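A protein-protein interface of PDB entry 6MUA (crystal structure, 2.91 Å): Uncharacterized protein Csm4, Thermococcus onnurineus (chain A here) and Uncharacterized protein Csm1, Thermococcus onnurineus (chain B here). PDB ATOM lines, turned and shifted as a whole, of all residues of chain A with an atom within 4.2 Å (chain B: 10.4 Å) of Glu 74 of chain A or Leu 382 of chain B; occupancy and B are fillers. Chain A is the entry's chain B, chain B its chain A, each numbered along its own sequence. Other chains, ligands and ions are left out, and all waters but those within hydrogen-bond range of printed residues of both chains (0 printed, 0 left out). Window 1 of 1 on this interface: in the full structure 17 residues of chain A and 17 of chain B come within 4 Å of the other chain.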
ATOM      1  N   LYS A  69     -17.936   2.238 -21.210  1.00  0.00           N
ATOM      2  CA  LYS A  69     -18.719   2.243 -19.955  1.00  0.00           C
ATOM      3  C   LYS A  69     -18.782   0.818 -19.413  1.00  0.00           C
ATOM      4  O   LYS A  69     -19.250  -0.050 -20.144  1.00  0.00           O
ATOM      5  CB  LYS A  69     -20.135   2.719 -20.281  1.00  0.00           C
ATOM      6  CG  LYS A  69     -21.083   2.863 -19.103  1.00  0.00           C
ATOM      7  CD  LYS A  69     -22.516   3.101 -19.506  1.00  0.00           C
ATOM      8  CE  LYS A  69     -23.437   3.314 -18.330  1.00  0.00           C
ATOM      9  NZ  LYS A  69     -23.159   4.600 -17.654  1.00  0.00           N
ATOM     10  N   LEU A  71     -20.325  -2.257 -17.515  1.00  0.00           N
ATOM     11  CA  LEU A  71     -21.720  -2.631 -17.283  1.00  0.00           C
ATOM     12  C   LEU A  71     -21.981  -2.756 -15.776  1.00  0.00           C
ATOM     13  O   LEU A  71     -23.121  -2.898 -15.365  1.00  0.00           O
ATOM     14  CB  LEU A  71     -22.027  -3.950 -18.002  1.00  0.00           C
ATOM     15  CG  LEU A  71     -21.748  -3.990 -19.506  1.00  0.00           C
ATOM     16  CD1 LEU A  71     -22.141  -5.338 -20.098  1.00  0.00           C
ATOM     17  CD2 LEU A  71     -22.472  -2.869 -20.231  1.00  0.00           C
ATOM     18  N   SER A  72     -20.931  -2.691 -14.959  1.00  0.00           N
ATOM     19  CA  SER A  72     -21.070  -2.774 -13.502  1.00  0.00           C
ATOM     20  C   SER A  72     -21.997  -1.667 -12.978  1.00  0.00           C
ATOM     21  O   SER A  72     -22.654  -1.859 -11.957  1.00  0.00           O
ATOM     22  CB  SER A  72     -19.712  -2.745 -12.800  1.00  0.00           C
ATOM     23  OG  SER A  72     -19.121  -1.448 -12.801  1.00  0.00           O
ATOM     24  N   VAL A  73     -22.056  -0.520 -13.654  1.00  0.00           N
ATOM     25  CA  VAL A  73     -22.808   0.618 -13.119  1.00  0.00           C
ATOM     26  C   VAL A  73     -24.290   0.502 -13.497  1.00  0.00           C
ATOM     27  O   VAL A  73     -25.100   1.214 -12.908  1.00  0.00           O
ATOM     28  CB  VAL A  73     -22.227   1.968 -13.582  1.00  0.00           C
ATOM     29  CG1 VAL A  73     -20.761   2.111 -13.205  1.00  0.00           C
ATOM     30  CG2 VAL A  73     -22.430   2.211 -15.073  1.00  0.00           C
ATOM     31  N   GLU A  74     -24.651  -0.364 -14.449  1.00  0.00           N
ATOM     32  CA  GLU A  74     -26.050  -0.432 -14.940  1.00  0.00           C
ATOM     33  C   GLU A  74     -26.993  -0.802 -13.789  1.00  0.00           C
ATOM     34  O   GLU A  74     -28.022  -0.151 -13.609  1.00  0.00           O
ATOM     35  CB  GLU A  74     -26.257  -1.458 -16.062  1.00  0.00           C
ATOM     36  CG  GLU A  74     -25.333  -1.308 -17.255  1.00  0.00           C
ATOM     37  CD  GLU A  74     -25.695  -0.182 -18.200  1.00  0.00           C
ATOM     38  OE1 GLU A  74     -25.977   0.924 -17.705  1.00  0.00           O
ATOM     39  OE2 GLU A  74     -25.681  -0.414 -19.427  1.00  0.00           O
ATOM     40  N   PRO A  75     -26.654  -1.852 -13.016  1.00  0.00           N
ATOM     41  CA  PRO A  75     -27.506  -2.250 -11.893  1.00  0.00           C
ATOM     42  C   PRO A  75     -27.420  -1.336 -10.661  1.00  0.00           C
ATOM     43  O   PRO A  75     -28.116  -1.599  -9.691  1.00  0.00           O
ATOM     44  CB  PRO A  75     -27.022  -3.651 -11.480  1.00  0.00           C
ATOM     45  CG  PRO A  75     -26.233  -4.127 -12.664  1.00  0.00           C
ATOM     46  CD  PRO A  75     -25.592  -2.854 -13.166  1.00  0.00           C
ATOM     47  N   ALA A  76     -26.608  -0.282 -10.698  1.00  0.00           N
ATOM     48  CA  ALA A  76     -26.306   0.502  -9.501  1.00  0.00           C
ATOM     49  C   ALA A  76     -26.730   1.967  -9.663  1.00  0.00           C
ATOM     50  O   ALA A  76     -26.405   2.800  -8.810  1.00  0.00           O
ATOM     51  CB  ALA A  76     -24.828   0.401  -9.211  1.00  0.00           C
ATOM     52  N   LEU A  77     -27.463   2.303 -10.716  1.00  0.00           N
ATOM     53  CA  LEU A  77     -27.676   3.721 -11.044  1.00  0.00           C
ATOM     54  C   LEU A  77     -28.496   4.422  -9.952  1.00  0.00           C
ATOM     55  O   LEU A  77     -28.406   5.645  -9.806  1.00  0.00           O
ATOM     56  CB  LEU A  77     -28.361   3.821 -12.409  1.00  0.00           C
ATOM     57  CG  LEU A  77     -27.494   3.382 -13.587  1.00  0.00           C
ATOM     58  CD1 LEU A  77     -28.338   2.994 -14.791  1.00  0.00           C
ATOM     59  CD2 LEU A  77     -26.498   4.465 -13.959  1.00  0.00           C
ATOM     60  N   ARG A  97     -27.630   4.727 -19.256  1.00  0.00           N
ATOM     61  CA  ARG A  97     -27.706   3.329 -19.682  1.00  0.00           C
ATOM     62  C   ARG A  97     -27.388   3.227 -21.181  1.00  0.00           C
ATOM     63  O   ARG A  97     -26.886   2.200 -21.643  1.00  0.00           O
ATOM     64  CB  ARG A  97     -29.097   2.768 -19.360  1.00  0.00           C
ATOM     65  CG  ARG A  97     -29.252   1.273 -19.612  1.00  0.00           C
ATOM     66  CD  ARG A  97     -30.638   0.740 -19.276  1.00  0.00           C
ATOM     67  NE  ARG A  97     -31.075   1.054 -17.917  1.00  0.00           N
ATOM     68  CZ  ARG A  97     -30.765   0.347 -16.831  1.00  0.00           C
ATOM     69  NH1 ARG A  97     -31.293   0.669 -15.662  1.00  0.00           N
ATOM     70  NH2 ARG A  97     -29.928  -0.672 -16.914  1.00  0.00           N
ATOM     71  N   VAL A 225     -19.945 -12.479 -15.326  1.00  0.00           N
ATOM     72  CA  VAL A 225     -20.817 -11.858 -14.313  1.00  0.00           C
ATOM     73  C   VAL A 225     -21.904 -11.020 -15.006  1.00  0.00           C
ATOM     74  O   VAL A 225     -23.088 -11.287 -14.835  1.00  0.00           O
ATOM     75  CB  VAL A 225     -20.003 -11.003 -13.323  1.00  0.00           C
ATOM     76  CG1 VAL A 225     -20.889 -10.386 -12.251  1.00  0.00           C
ATOM     77  CG2 VAL A 225     -18.879 -11.798 -12.684  1.00  0.00           C
ATOM     78  N   LEU A 226     -21.493  -9.992 -15.751  1.00  0.00           N
ATOM     79  CA  LEU A 226     -22.403  -9.145 -16.532  1.00  0.00           C
ATOM     80  C   LEU A 226     -21.868  -9.051 -17.962  1.00  0.00           C
ATOM     81  O   LEU A 226     -20.665  -8.927 -18.131  1.00  0.00           O
ATOM     82  CB  LEU A 226     -22.466  -7.754 -15.896  1.00  0.00           C
ATOM     83  CG  LEU A 226     -23.161  -7.664 -14.539  1.00  0.00           C
ATOM     84  CD1 LEU A 226     -22.902  -6.312 -13.884  1.00  0.00           C
ATOM     85  CD2 LEU A 226     -24.653  -7.912 -14.678  1.00  0.00           C
ATOM     86  N   TRP A 227     -22.725  -9.082 -18.983  1.00  0.00           N
ATOM     87  CA  TRP A 227     -22.191  -9.049 -20.340  1.00  0.00           C
ATOM     88  C   TRP A 227     -23.194  -8.532 -21.370  1.00  0.00           C
ATOM     89  O   TRP A 227     -24.393  -8.415 -21.116  1.00  0.00           O
ATOM     90  CB  TRP A 227     -21.671 -10.433 -20.736  1.00  0.00           C
ATOM     91  CG  TRP A 227     -22.682 -11.502 -21.024  1.00  0.00           C
ATOM     92  CD1 TRP A 227     -23.205 -11.827 -22.244  1.00  0.00           C
ATOM     93  CD2 TRP A 227     -23.183 -12.493 -20.110  1.00  0.00           C
ATOM     94  NE1 TRP A 227     -24.025 -12.920 -22.144  1.00  0.00           N
ATOM     95  CE2 TRP A 227     -24.033 -13.349 -20.844  1.00  0.00           C
ATOM     96  CE3 TRP A 227     -23.020 -12.728 -18.738  1.00  0.00           C
ATOM     97  CZ2 TRP A 227     -24.709 -14.417 -20.253  1.00  0.00           C
ATOM     98  CZ3 TRP A 227     -23.677 -13.792 -18.160  1.00  0.00           C
ATOM     99  CH2 TRP A 227     -24.516 -14.619 -18.907  1.00  0.00           C
ATOM    100  N   ASP B 253     -40.145 -10.219 -19.661  1.00  0.00           N
ATOM    101  CA  ASP B 253     -39.904  -9.147 -20.607  1.00  0.00           C
ATOM    102  C   ASP B 253     -38.963  -9.654 -21.705  1.00  0.00           C
ATOM    103  O   ASP B 253     -37.959 -10.302 -21.413  1.00  0.00           O
ATOM    104  CB  ASP B 253     -39.331  -7.927 -19.885  1.00  0.00           C
ATOM    105  CG  ASP B 253     -39.022  -6.760 -20.805  1.00  0.00           C
ATOM    106  OD1 ASP B 253     -39.946  -5.960 -21.071  1.00  0.00           O
ATOM    107  OD2 ASP B 253     -37.861  -6.662 -21.247  1.00  0.00           O
ATOM    108  N   SER B 255     -36.248  -8.968 -24.795  1.00  0.00           N
ATOM    109  CA  SER B 255     -35.255  -7.973 -25.194  1.00  0.00           C
ATOM    110  C   SER B 255     -34.668  -8.359 -26.556  1.00  0.00           C
ATOM    111  O   SER B 255     -34.328  -9.517 -26.802  1.00  0.00           O
ATOM    112  CB  SER B 255     -34.188  -7.788 -24.143  1.00  0.00           C
ATOM    113  OG  SER B 255     -33.315  -8.900 -24.105  1.00  0.00           O
ATOM    114  N   TYR B 344     -34.337 -12.510 -26.919  1.00  0.00           N
ATOM    115  CA  TYR B 344     -34.122 -13.140 -25.618  1.00  0.00           C
ATOM    116  C   TYR B 344     -35.340 -12.898 -24.720  1.00  0.00           C
ATOM    117  O   TYR B 344     -35.979 -11.854 -24.820  1.00  0.00           O
ATOM    118  CB  TYR B 344     -32.868 -12.556 -24.968  1.00  0.00           C
ATOM    119  CG  TYR B 344     -32.644 -12.977 -23.542  1.00  0.00           C
ATOM    120  CD1 TYR B 344     -32.526 -14.315 -23.208  1.00  0.00           C
ATOM    121  CD2 TYR B 344     -32.534 -12.043 -22.526  1.00  0.00           C
ATOM    122  CE1 TYR B 344     -32.308 -14.714 -21.900  1.00  0.00           C
ATOM    123  CE2 TYR B 344     -32.319 -12.425 -21.211  1.00  0.00           C
ATOM    124  CZ  TYR B 344     -32.201 -13.765 -20.900  1.00  0.00           C
ATOM    125  OH  TYR B 344     -31.982 -14.157 -19.614  1.00  0.00           O
ATOM    126  N   LEU B 345     -35.647 -13.854 -23.850  1.00  0.00           N
ATOM    127  CA  LEU B 345     -36.735 -13.698 -22.890  1.00  0.00           C
ATOM    128  C   LEU B 345     -36.165 -13.671 -21.466  1.00  0.00           C
ATOM    129  O   LEU B 345     -35.778 -14.705 -20.904  1.00  0.00           O
ATOM    130  CB  LEU B 345     -37.740 -14.842 -23.073  1.00  0.00           C
ATOM    131  CG  LEU B 345     -38.964 -14.824 -22.152  1.00  0.00           C
ATOM    132  CD1 LEU B 345     -39.743 -13.523 -22.281  1.00  0.00           C
ATOM    133  CD2 LEU B 345     -39.874 -16.009 -22.443  1.00  0.00           C
ATOM    134  N   ALA B 346     -36.120 -12.478 -20.891  1.00  0.00           N
ATOM    135  CA  ALA B 346     -35.708 -12.334 -19.509  1.00  0.00           C
ATOM    136  C   ALA B 346     -36.915 -12.622 -18.619  1.00  0.00           C
ATOM    137  O   ALA B 346     -37.961 -12.045 -18.839  1.00  0.00           O
ATOM    138  CB  ALA B 346     -35.171 -10.944 -19.270  1.00  0.00           C
ATOM    139  N   ILE B 347     -36.773 -13.518 -17.650  1.00  0.00           N
ATOM    140  CA  ILE B 347     -37.873 -13.818 -16.718  1.00  0.00           C
ATOM    141  C   ILE B 347     -37.319 -13.851 -15.292  1.00  0.00           C
ATOM    142  O   ILE B 347     -36.277 -14.462 -15.026  1.00  0.00           O
ATOM    143  CB  ILE B 347     -38.583 -15.148 -17.047  1.00  0.00           C
ATOM    144  CG1 ILE B 347     -39.032 -15.230 -18.510  1.00  0.00           C
ATOM    145  CG2 ILE B 347     -39.741 -15.363 -16.085  1.00  0.00           C
ATOM    146  CD1 ILE B 347     -39.655 -16.553 -18.894  1.00  0.00           C
ATOM    147  N   GLU B 348     -38.055 -13.220 -14.388  1.00  0.00           N
ATOM    148  CA  GLU B 348     -37.716 -13.246 -12.979  1.00  0.00           C
ATOM    149  C   GLU B 348     -39.012 -13.217 -12.162  1.00  0.00           C
ATOM    150  O   GLU B 348     -40.097 -13.022 -12.698  1.00  0.00           O
ATOM    151  CB  GLU B 348     -36.784 -12.083 -12.626  1.00  0.00           C
ATOM    152  CG  GLU B 348     -35.318 -12.332 -12.965  1.00  0.00           C
ATOM    153  CD  GLU B 348     -34.650 -13.502 -12.256  1.00  0.00           C
ATOM    154  OE1 GLU B 348     -33.599 -13.961 -12.749  1.00  0.00           O
ATOM    155  OE2 GLU B 348     -35.176 -13.951 -11.212  1.00  0.00           O
ATOM    156  N   LYS B 374     -37.994  -5.337 -10.975  1.00  0.00           N
ATOM    157  CA  LYS B 374     -37.432  -4.674 -12.158  1.00  0.00           C
ATOM    158  C   LYS B 374     -35.905  -4.827 -12.136  1.00  0.00           C
ATOM    159  O   LYS B 374     -35.284  -5.054 -13.169  1.00  0.00           O
ATOM    160  CB  LYS B 374     -37.838  -3.195 -12.200  1.00  0.00           C
ATOM    161  CG  LYS B 374     -37.217  -2.375 -13.327  1.00  0.00           C
ATOM    162  CD  LYS B 374     -37.800  -2.669 -14.704  1.00  0.00           C
ATOM    163  CE  LYS B 374     -36.818  -2.520 -15.851  1.00  0.00           C
ATOM    164  NZ  LYS B 374     -36.272  -3.826 -16.303  1.00  0.00           N
ATOM    165  N   HIS B 375     -35.317  -4.718 -10.951  1.00  0.00           N
ATOM    166  CA  HIS B 375     -33.875  -4.848 -10.784  1.00  0.00           C
ATOM    167  C   HIS B 375     -33.421  -6.266 -11.153  1.00  0.00           C
ATOM    168  O   HIS B 375     -32.500  -6.433 -11.949  1.00  0.00           O
ATOM    169  CB  HIS B 375     -33.469  -4.472  -9.352  1.00  0.00           C
ATOM    170  CG  HIS B 375     -31.993  -4.398  -9.157  1.00  0.00           C
ATOM    171  ND1 HIS B 375     -31.278  -5.419  -8.560  1.00  0.00           N
ATOM    172  CD2 HIS B 375     -31.097  -3.445  -9.493  1.00  0.00           C
ATOM    173  CE1 HIS B 375     -30.002  -5.091  -8.523  1.00  0.00           C
ATOM    174  NE2 HIS B 375     -29.865  -3.883  -9.090  1.00  0.00           N
ATOM    175  N   LYS B 376     -34.055  -7.283 -10.574  1.00  0.00           N
ATOM    176  CA  LYS B 376     -33.752  -8.666 -10.948  1.00  0.00           C
ATOM    177  C   LYS B 376     -33.813  -8.802 -12.477  1.00  0.00           C
ATOM    178  O   LYS B 376     -33.023  -9.534 -13.079  1.00  0.00           O
ATOM    179  CB  LYS B 376     -34.744  -9.656 -10.327  1.00  0.00           C
ATOM    180  CG  LYS B 376     -34.650  -9.856  -8.821  1.00  0.00           C
ATOM    181  CD  LYS B 376     -35.193 -11.207  -8.374  1.00  0.00           C
ATOM    182  CE  LYS B 376     -35.842 -11.189  -7.004  1.00  0.00           C
ATOM    183  NZ  LYS B 376     -34.853 -11.311  -5.908  1.00  0.00           N
ATOM    184  N   LEU B 377     -34.765  -8.085 -13.080  1.00  0.00           N
ATOM    185  CA  LEU B 377     -35.067  -8.197 -14.504  1.00  0.00           C
ATOM    186  C   LEU B 377     -34.005  -7.455 -15.334  1.00  0.00           C
ATOM    187  O   LEU B 377     -33.591  -7.966 -16.374  1.00  0.00           O
ATOM    188  CB  LEU B 377     -36.483  -7.653 -14.749  1.00  0.00           C
ATOM    189  CG  LEU B 377     -37.622  -8.441 -14.097  1.00  0.00           C
ATOM    190  CD1 LEU B 377     -38.954  -7.735 -14.282  1.00  0.00           C
ATOM    191  CD2 LEU B 377     -37.699  -9.856 -14.655  1.00  0.00           C
ATOM    192  N   THR B 378     -33.550  -6.274 -14.900  1.00  0.00           N
ATOM    193  CA  THR B 378     -32.422  -5.610 -15.577  1.00  0.00           C
ATOM    194  C   THR B 378     -31.171  -6.493 -15.499  1.00  0.00           C
ATOM    195  O   THR B 378     -30.506  -6.711 -16.501  1.00  0.00           O
ATOM    196  CB  THR B 378     -32.045  -4.252 -14.969  1.00  0.00           C
ATOM    197  OG1 THR B 378     -31.703  -4.477 -13.602  1.00  0.00           O
ATOM    198  CG2 THR B 378     -33.133  -3.207 -15.076  1.00  0.00           C
ATOM    199  N   VAL B 379     -30.849  -6.982 -14.306  1.00  0.00           N
ATOM    200  CA  VAL B 379     -29.649  -7.792 -14.114  1.00  0.00           C
ATOM    201  C   VAL B 379     -29.706  -8.986 -15.073  1.00  0.00           C
ATOM    202  O   VAL B 379     -28.691  -9.346 -15.656  1.00  0.00           O
ATOM    203  CB  VAL B 379     -29.479  -8.255 -12.651  1.00  0.00           C
ATOM    204  CG1 VAL B 379     -28.384  -9.301 -12.506  1.00  0.00           C
ATOM    205  CG2 VAL B 379     -29.211  -7.091 -11.708  1.00  0.00           C
ATOM    206  N   ARG B 380     -30.882  -9.582 -15.249  1.00  0.00           N
ATOM    207  CA  ARG B 380     -31.014 -10.776 -16.089  1.00  0.00           C
ATOM    208  C   ARG B 380     -30.793 -10.415 -17.572  1.00  0.00           C
ATOM    209  O   ARG B 380     -30.278 -11.241 -18.341  1.00  0.00           O
ATOM    210  CB  ARG B 380     -32.372 -11.438 -15.829  1.00  0.00           C
ATOM    211  CG  ARG B 380     -32.711 -12.606 -16.745  1.00  0.00           C
ATOM    212  CD  ARG B 380     -31.702 -13.732 -16.697  1.00  0.00           C
ATOM    213  NE  ARG B 380     -31.762 -14.493 -15.460  1.00  0.00           N
ATOM    214  CZ  ARG B 380     -30.931 -15.484 -15.152  1.00  0.00           C
ATOM    215  NH1 ARG B 380     -29.946 -15.803 -15.979  1.00  0.00           N
ATOM    216  NH2 ARG B 380     -31.088 -16.146 -14.017  1.00  0.00           N
ATOM    217  N   LYS B 381     -31.158  -9.199 -17.986  1.00  0.00           N
ATOM    218  CA  LYS B 381     -30.887  -8.741 -19.364  1.00  0.00           C
ATOM    219  C   LYS B 381     -29.380  -8.524 -19.579  1.00  0.00           C
ATOM    220  O   LYS B 381     -28.910  -8.555 -20.713  1.00  0.00           O
ATOM    221  CB  LYS B 381     -31.645  -7.446 -19.670  1.00  0.00           C
ATOM    222  CG  LYS B 381     -33.163  -7.554 -19.667  1.00  0.00           C
ATOM    223  CD  LYS B 381     -33.847  -6.295 -20.163  1.00  0.00           C
ATOM    224  CE  LYS B 381     -35.102  -5.942 -19.394  1.00  0.00           C
ATOM    225  NZ  LYS B 381     -35.624  -4.613 -19.795  1.00  0.00           N
ATOM    226  N   LEU B 382     -28.630  -8.292 -18.503  1.00  0.00           N
ATOM    227  CA  LEU B 382     -27.166  -8.233 -18.557  1.00  0.00           C
ATOM    228  C   LEU B 382     -26.566  -9.622 -18.295  1.00  0.00           C
ATOM    229  O   LEU B 382     -25.423  -9.719 -17.845  1.00  0.00           O
ATOM    230  CB  LEU B 382     -26.656  -7.233 -17.513  1.00  0.00           C
ATOM    231  CG  LEU B 382     -27.066  -5.778 -17.713  1.00  0.00           C
ATOM    232  CD1 LEU B 382     -26.606  -4.937 -16.536  1.00  0.00           C
ATOM    233  CD2 LEU B 382     -26.505  -5.215 -19.010  1.00  0.00           C
ATOM    234  N   LYS B 383     -27.335 -10.682 -18.545  1.00  0.00           N
ATOM    235  CA  LYS B 383     -26.833 -12.055 -18.523  1.00  0.00           C
ATOM    236  C   LYS B 383     -27.594 -12.850 -19.589  1.00  0.00           C
ATOM    237  O   LYS B 383     -28.121 -13.937 -19.315  1.00  0.00           O
ATOM    238  CB  LYS B 383     -27.002 -12.676 -17.130  1.00  0.00           C
ATOM    239  CG  LYS B 383     -26.388 -11.893 -15.971  1.00  0.00           C
ATOM    240  CD  LYS B 383     -26.854 -12.331 -14.597  1.00  0.00           C
ATOM    241  CE  LYS B 383     -26.198 -13.607 -14.118  1.00  0.00           C
ATOM    242  NZ  LYS B 383     -24.976 -13.322 -13.331  1.00  0.00           N
ATOM    243  N   ARG B 384     -27.656 -12.266 -20.773  1.00  0.00           N
ATOM    244  CA  ARG B 384     -28.486 -12.889 -21.825  1.00  0.00           C
ATOM    245  C   ARG B 384     -28.002 -14.316 -22.072  1.00  0.00           C
ATOM    246  O   ARG B 384     -26.809 -14.524 -22.370  1.00  0.00           O
ATOM    247  CB  ARG B 384     -28.420 -12.060 -23.112  1.00  0.00           C
ATOM    248  CG  ARG B 384     -28.917 -10.630 -22.955  1.00  0.00           C
ATOM    249  CD  ARG B 384     -28.884  -9.857 -24.260  1.00  0.00           C
ATOM    250  NE  ARG B 384     -29.741 -10.451 -25.277  1.00  0.00           N
ATOM    251  CZ  ARG B 384     -29.902  -9.964 -26.503  1.00  0.00           C
ATOM    252  NH1 ARG B 384     -29.263  -8.866 -26.868  1.00  0.00           N
ATOM    253  NH2 ARG B 384     -30.703 -10.576 -27.357  1.00  0.00           N
ATOM    254  N   PHE B 385     -28.946 -15.230 -21.960  1.00  0.00           N
ATOM    255  CA  PHE B 385     -28.764 -16.645 -22.278  1.00  0.00           C
ATOM    256  C   PHE B 385     -27.808 -17.308 -21.278  1.00  0.00           C
ATOM    257  O   PHE B 385     -27.187 -18.304 -21.622  1.00  0.00           O
ATOM    258  CB  PHE B 385     -28.267 -16.845 -23.713  1.00  0.00           C
ATOM    259  CG  PHE B 385     -29.216 -16.370 -24.782  1.00  0.00           C
ATOM    260  CD1 PHE B 385     -30.230 -17.194 -25.248  1.00  0.00           C
ATOM    261  CD2 PHE B 385     -29.088 -15.108 -25.332  1.00  0.00           C
ATOM    262  CE1 PHE B 385     -31.099 -16.760 -26.238  1.00  0.00           C
ATOM    263  CE2 PHE B 385     -29.957 -14.675 -26.323  1.00  0.00           C
ATOM    264  CZ  PHE B 385     -30.959 -15.502 -26.776  1.00  0.00           C
ATOM    265  N   GLY B 386     -27.733 -16.793 -20.048  1.00  0.00           N
ATOM    266  CA  GLY B 386     -26.961 -17.438 -18.985  1.00  0.00           C
ATOM    267  C   GLY B 386     -27.589 -18.741 -18.506  1.00  0.00           C
ATOM    268  O   GLY B 386     -27.140 -19.310 -17.516  1.00  0.00           O
ATOM    269  N   GLU B 387     -28.628 -19.208 -19.201  1.00  0.00           N
ATOM    270  CA  GLU B 387     -29.287 -20.486 -18.934  1.00  0.00           C
ATOM    271  C   GLU B 387     -28.901 -21.497 -20.024  1.00  0.00           C
ATOM    272  O   GLU B 387     -29.578 -22.509 -20.223  1.00  0.00           O
ATOM    273  CB  GLU B 387     -30.803 -20.269 -18.881  1.00  0.00           C
ATOM    274  CG  GLU B 387     -31.226 -19.129 -17.962  1.00  0.00           C
ATOM    275  CD  GLU B 387     -31.525 -17.788 -18.623  1.00  0.00           C
ATOM    276  OE1 GLU B 387     -31.953 -16.865 -17.900  1.00  0.00           O
ATOM    277  OE2 GLU B 387     -31.334 -17.660 -19.853  1.00  0.00           O
ATOM    278  N   LEU B 391     -23.124 -21.933 -24.362  1.00  0.00           N
ATOM    279  CA  LEU B 391     -23.005 -20.647 -25.079  1.00  0.00           C
ATOM    280  C   LEU B 391     -21.526 -20.302 -25.238  1.00  0.00           C
ATOM    281  O   LEU B 391     -21.210 -19.529 -26.151  1.00  0.00           O
ATOM    282  CB  LEU B 391     -23.708 -19.588 -24.234  1.00  0.00           C
ATOM    283  CG  LEU B 391     -23.829 -18.224 -24.892  1.00  0.00           C
ATOM    284  CD1 LEU B 391     -24.579 -18.341 -26.205  1.00  0.00           C
ATOM    285  CD2 LEU B 391     -24.531 -17.267 -23.956  1.00  0.00           C
ATOM    286  N   PHE B 392     -20.670 -20.789 -24.353  1.00  0.00           N
ATOM    287  CA  PHE B 392     -19.255 -20.441 -24.433  1.00  0.00           C
ATOM    288  C   PHE B 392     -18.432 -21.712 -24.686  1.00  0.00           C
ATOM    289  O   PHE B 392     -17.580 -22.097 -23.877  1.00  0.00           O
ATOM    290  CB  PHE B 392     -18.852 -19.678 -23.168  1.00  0.00           C
ATOM    291  CG  PHE B 392     -19.636 -18.406 -22.949  1.00  0.00           C
ATOM    292  CD1 PHE B 392     -19.771 -17.474 -23.970  1.00  0.00           C
ATOM    293  CD2 PHE B 392     -20.234 -18.134 -21.727  1.00  0.00           C
ATOM    294  CE1 PHE B 392     -20.485 -16.302 -23.773  1.00  0.00           C
ATOM    295  CE2 PHE B 392     -20.950 -16.962 -21.533  1.00  0.00           C
ATOM    296  CZ  PHE B 392     -21.074 -16.049 -22.555  1.00  0.00           C
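Among the printed residues, pairs that only touch across the chains: Glu 74 of chain A with Leu 382 of chain B, Pro 75 of chain A with Leu 382 of chain B, Leu 226 of chain A with Leu 382 of chain B, Trp 227 of chain A with Lys 383 of chain B and Trp 227 of chain A with Gly 386 of chain B.
O of His 375 of chain B is in hydrogen-bond range of OG1 of Thr 378 of chain B (2.7 Å).
O of Arg 384 of chain B lies close to NE1 of Trp 227 of chain A (3.2 Å). A ring nitrogen (NE2) of His 375 of chain B lies within hydrogen-bond range of the backbone carbonyl oxygen (O) of Pro 75 of chain A, 2.9 Å away. O of Leu 382 of chain B lies within hydrogen-bond range of N of Trp 227 of chain A (3.0 Å). The side-chain amino group of Lys 383 of chain B lies within hydrogen-bond range of the backbone carbonyl oxygen of Val 225 of chain A (3.2 Å).
Of the 23 printed residues of chain B, 5 touch a printed residue of chain A. Hydrophobic or aromatic side chains of chain B within 4 Å of the printed part of chain A: His 375 and Leu 382. Hydrophobic or aromatic side chains of chain A within 4 Å of the printed part of chain B: Pro 75, Leu 226 and Trp 227. Along chain A the printed residues that touch a printed residue of chain B span positions 74 to 227. Among the printed residues, no Asp or Glu carboxylate lies within 4 Å of a Lys or Arg side-chain nitrogen of the other chain.
No residue of chain B comes within 4 Å of Leu 71 of chain A. No residue of chain B comes within 4 Å of Val 73 of chain A. Glu 74 of chain A touches one residue of chain B. Of the printed residues of chain B, Pro 75 of chain A touches His 375 and Leu 382. No residue of chain B comes within 4 Å of Arg 97 of chain A. Printed residues of chain B within 4 Å of Trp 227 of chain A: Leu 382 (3.0 Å), Lys 383 (3.3 Å), Arg 384 (3.0 Å) and Gly 386 (3.7 Å). Printed residues of chain A within 4 Å of Leu 382 of chain B: Glu 74 (3.5 Å), Pro 75 (3.97 Å), Leu 226 (3.3 Å) and Trp 227 (3.0 Å). Of the printed residues of chain A, Lys 383 of chain B touches Val 225 and Trp 227. Printed residues of chain A within 4 Å of Arg 384 of chain B: Trp 227. The nearest residue of chain B that does not touch Glu 74 of chain A is Thr 378 of chain B (5.7 Å). The nearest residue of chain A that does not touch Leu 382 of chain B is Val 225 of chain A (4.1 Å). The nearest printed residue of chain A that does not touch His 375 of chain B is Ala 76 of chain A (5.1 Å).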
